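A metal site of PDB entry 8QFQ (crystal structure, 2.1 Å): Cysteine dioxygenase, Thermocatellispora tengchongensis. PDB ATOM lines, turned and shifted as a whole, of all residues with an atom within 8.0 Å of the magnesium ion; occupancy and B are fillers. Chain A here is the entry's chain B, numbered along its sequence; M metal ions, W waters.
The side-chain carboxylate (OD1) of Asp 69 is in hydrogen-bond range of the backbone NH (N) of Val 72 (2.9 Å).
The backbone NH (N) of Tyr 71 sits at hydrogen-bond distance from the side-chain carboxylate (OD1) of Asp 69 (2.8 Å).
NE2 of His 67 is bound to the magnesium ion (1.9 Å).
OD2 of Asp 69 is bound to the magnesium ion (2.0 Å).
The magnesium ion is bound by water W1 (2.1 Å).
OE1 of Glu 22 binds the magnesium ion (2.2 Å).
The magnesium ion has four donor atoms within binding distance.
Of the 12 residues printed, 3 come within 4 Å of the magnesium ion.
The nearest printed residue that does not touch the magnesium ion is Leu 23 (4.4 Å).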
ATOM      1  N   GLU A  22      16.289  22.531 -12.536  1.00  0.00           N
ATOM      2  CA  GLU A  22      15.171  23.263 -13.137  1.00  0.00           C
ATOM      3  C   GLU A  22      14.696  24.412 -12.252  1.00  0.00           C
ATOM      4  O   GLU A  22      14.544  24.239 -11.052  1.00  0.00           O
ATOM      5  CB  GLU A  22      14.016  22.285 -13.444  1.00  0.00           C
ATOM      6  CG  GLU A  22      12.908  22.838 -14.389  1.00  0.00           C
ATOM      7  CD  GLU A  22      13.449  23.535 -15.658  1.00  0.00           C
ATOM      8  OE1 GLU A  22      13.508  24.792 -15.664  1.00  0.00           O
ATOM      9  OE2 GLU A  22      13.878  22.878 -16.632  1.00  0.00           O
ATOM     10  N   LEU A  23      14.357  25.547 -12.861  1.00  0.00           N
ATOM     11  CA  LEU A  23      13.912  26.697 -12.088  1.00  0.00           C
ATOM     12  C   LEU A  23      12.488  27.022 -12.493  1.00  0.00           C
ATOM     13  O   LEU A  23      12.175  27.105 -13.675  1.00  0.00           O
ATOM     14  CB  LEU A  23      14.800  27.920 -12.355  1.00  0.00           C
ATOM     15  CG  LEU A  23      16.273  27.754 -11.977  1.00  0.00           C
ATOM     16  CD1 LEU A  23      17.097  28.838 -12.629  1.00  0.00           C
ATOM     17  CD2 LEU A  23      16.484  27.678 -10.430  1.00  0.00           C
ATOM     18  N   ASP A  24      11.649  27.236 -11.496  1.00  0.00           N
ATOM     19  CA  ASP A  24      10.250  27.617 -11.638  1.00  0.00           C
ATOM     20  C   ASP A  24      10.239  29.074 -12.043  1.00  0.00           C
ATOM     21  O   ASP A  24      10.343  29.958 -11.187  1.00  0.00           O
ATOM     22  CB  ASP A  24       9.505  27.371 -10.319  1.00  0.00           C
ATOM     23  CG  ASP A  24       7.978  27.504 -10.457  1.00  0.00           C
ATOM     24  OD1 ASP A  24       7.492  27.977 -11.512  1.00  0.00           O
ATOM     25  OD2 ASP A  24       7.249  27.142  -9.499  1.00  0.00           O
ATOM     26  N   LEU A  25      10.134  29.333 -13.346  1.00  0.00           N
ATOM     27  CA  LEU A  25      10.156  30.670 -13.912  1.00  0.00           C
ATOM     28  C   LEU A  25       9.076  30.772 -14.972  1.00  0.00           C
ATOM     29  O   LEU A  25       8.743  29.768 -15.604  1.00  0.00           O
ATOM     30  CB  LEU A  25      11.507  30.976 -14.589  1.00  0.00           C
ATOM     31  CG  LEU A  25      12.674  31.116 -13.606  1.00  0.00           C
ATOM     32  CD1 LEU A  25      13.976  31.067 -14.388  1.00  0.00           C
ATOM     33  CD2 LEU A  25      12.550  32.336 -12.705  1.00  0.00           C
ATOM     34  N   PRO A  26       8.619  31.966 -15.277  1.00  0.00           N
ATOM     35  CA  PRO A  26       7.713  32.090 -16.422  1.00  0.00           C
ATOM     36  C   PRO A  26       8.384  31.591 -17.685  1.00  0.00           C
ATOM     37  O   PRO A  26       9.595  31.764 -17.872  1.00  0.00           O
ATOM     38  CB  PRO A  26       7.408  33.593 -16.480  1.00  0.00           C
ATOM     39  CG  PRO A  26       8.259  34.251 -15.406  1.00  0.00           C
ATOM     40  CD  PRO A  26       8.864  33.225 -14.541  1.00  0.00           C
ATOM     41  N   GLU A  27       7.584  31.062 -18.596  1.00  0.00           N
ATOM     42  CA  GLU A  27       8.116  30.459 -19.826  1.00  0.00           C
ATOM     43  C   GLU A  27       8.268  31.515 -20.922  1.00  0.00           C
ATOM     44  O   GLU A  27       7.609  31.486 -21.959  1.00  0.00           O
ATOM     45  CB  GLU A  27       7.183  29.339 -20.288  1.00  0.00           C
ATOM     46  CG  GLU A  27       7.143  28.151 -19.334  1.00  0.00           C
ATOM     47  CD  GLU A  27       6.245  28.406 -18.115  1.00  0.00           C
ATOM     48  OE1 GLU A  27       5.439  29.358 -18.132  1.00  0.00           O
ATOM     49  OE2 GLU A  27       6.346  27.620 -17.140  1.00  0.00           O
ATOM     50  N   HIS A  67      21.696  26.870 -14.492  1.00  0.00           N
ATOM     51  CA  HIS A  67      20.559  26.442 -15.315  1.00  0.00           C
ATOM     52  C   HIS A  67      20.695  27.208 -16.620  1.00  0.00           C
ATOM     53  O   HIS A  67      21.022  28.401 -16.629  1.00  0.00           O
ATOM     54  CB  HIS A  67      19.186  26.767 -14.653  1.00  0.00           C
ATOM     55  CG  HIS A  67      17.960  26.222 -15.382  1.00  0.00           C
ATOM     56  ND1 HIS A  67      17.787  24.881 -15.616  1.00  0.00           N
ATOM     57  CD2 HIS A  67      16.868  26.838 -15.956  1.00  0.00           C
ATOM     58  CE1 HIS A  67      16.624  24.700 -16.264  1.00  0.00           C
ATOM     59  NE2 HIS A  67      16.042  25.867 -16.490  1.00  0.00           N
ATOM     60  N   ARG A  68      20.470  26.499 -17.723  1.00  0.00           N
ATOM     61  CA  ARG A  68      20.479  27.073 -19.053  1.00  0.00           C
ATOM     62  C   ARG A  68      19.322  26.420 -19.786  1.00  0.00           C
ATOM     63  O   ARG A  68      19.206  25.191 -19.796  1.00  0.00           O
ATOM     64  CB  ARG A  68      21.798  26.833 -19.761  1.00  0.00           C
ATOM     65  CG  ARG A  68      22.990  27.127 -18.882  1.00  0.00           C
ATOM     66  CD  ARG A  68      24.236  26.881 -19.699  1.00  0.00           C
ATOM     67  NE  ARG A  68      24.179  27.670 -20.915  1.00  0.00           N
ATOM     68  CZ  ARG A  68      25.127  27.640 -21.841  1.00  0.00           C
ATOM     69  NH1 ARG A  68      26.161  26.845 -21.662  1.00  0.00           N
ATOM     70  NH2 ARG A  68      25.022  28.392 -22.935  1.00  0.00           N
ATOM     71  N   ASP A  69      18.441  27.238 -20.365  1.00  0.00           N
ATOM     72  CA  ASP A  69      17.314  26.748 -21.152  1.00  0.00           C
ATOM     73  C   ASP A  69      17.031  27.777 -22.232  1.00  0.00           C
ATOM     74  O   ASP A  69      17.915  28.582 -22.555  1.00  0.00           O
ATOM     75  CB  ASP A  69      16.145  26.415 -20.205  1.00  0.00           C
ATOM     76  CG  ASP A  69      15.521  27.645 -19.549  1.00  0.00           C
ATOM     77  OD1 ASP A  69      15.751  28.807 -19.995  1.00  0.00           O
ATOM     78  OD2 ASP A  69      14.826  27.436 -18.525  1.00  0.00           O
ATOM     79  N   ALA A  70      15.853  27.722 -22.836  1.00  0.00           N
ATOM     80  CA  ALA A  70      15.651  28.591 -23.984  1.00  0.00           C
ATOM     81  C   ALA A  70      15.578  30.066 -23.569  1.00  0.00           C
ATOM     82  O   ALA A  70      15.748  30.950 -24.411  1.00  0.00           O
ATOM     83  CB  ALA A  70      14.350  28.221 -24.732  1.00  0.00           C
ATOM     84  N   TYR A  71      15.325  30.335 -22.283  1.00  0.00           N
ATOM     85  CA  TYR A  71      15.023  31.680 -21.822  1.00  0.00           C
ATOM     86  C   TYR A  71      16.109  32.315 -20.974  1.00  0.00           C
ATOM     87  O   TYR A  71      16.318  33.522 -21.070  1.00  0.00           O
ATOM     88  CB  TYR A  71      13.707  31.664 -21.011  1.00  0.00           C
ATOM     89  CG  TYR A  71      12.575  31.067 -21.804  1.00  0.00           C
ATOM     90  CD1 TYR A  71      12.114  31.671 -22.963  1.00  0.00           C
ATOM     91  CD2 TYR A  71      11.998  29.856 -21.400  1.00  0.00           C
ATOM     92  CE1 TYR A  71      11.078  31.118 -23.715  1.00  0.00           C
ATOM     93  CE2 TYR A  71      10.984  29.262 -22.143  1.00  0.00           C
ATOM     94  CZ  TYR A  71      10.515  29.898 -23.296  1.00  0.00           C
ATOM     95  OH  TYR A  71       9.482  29.302 -24.002  1.00  0.00           O
ATOM     96  N   VAL A  72      16.807  31.529 -20.132  1.00  0.00           N
ATOM     97  CA  VAL A  72      17.790  32.065 -19.201  1.00  0.00           C
ATOM     98  C   VAL A  72      19.087  31.256 -19.230  1.00  0.00           C
ATOM     99  O   VAL A  72      19.100  30.054 -19.516  1.00  0.00           O
ATOM    100  CB  VAL A  72      17.242  32.075 -17.731  1.00  0.00           C
ATOM    101  CG1 VAL A  72      15.902  32.819 -17.665  1.00  0.00           C
ATOM    102  CG2 VAL A  72      17.094  30.651 -17.196  1.00  0.00           C
HETATM  103 MG    MG M   1      14.291  25.945 -17.316  1.00  0.00          MG
HETATM  104  O   HOH W   1      13.619  27.506 -16.000  1.00  0.00           O
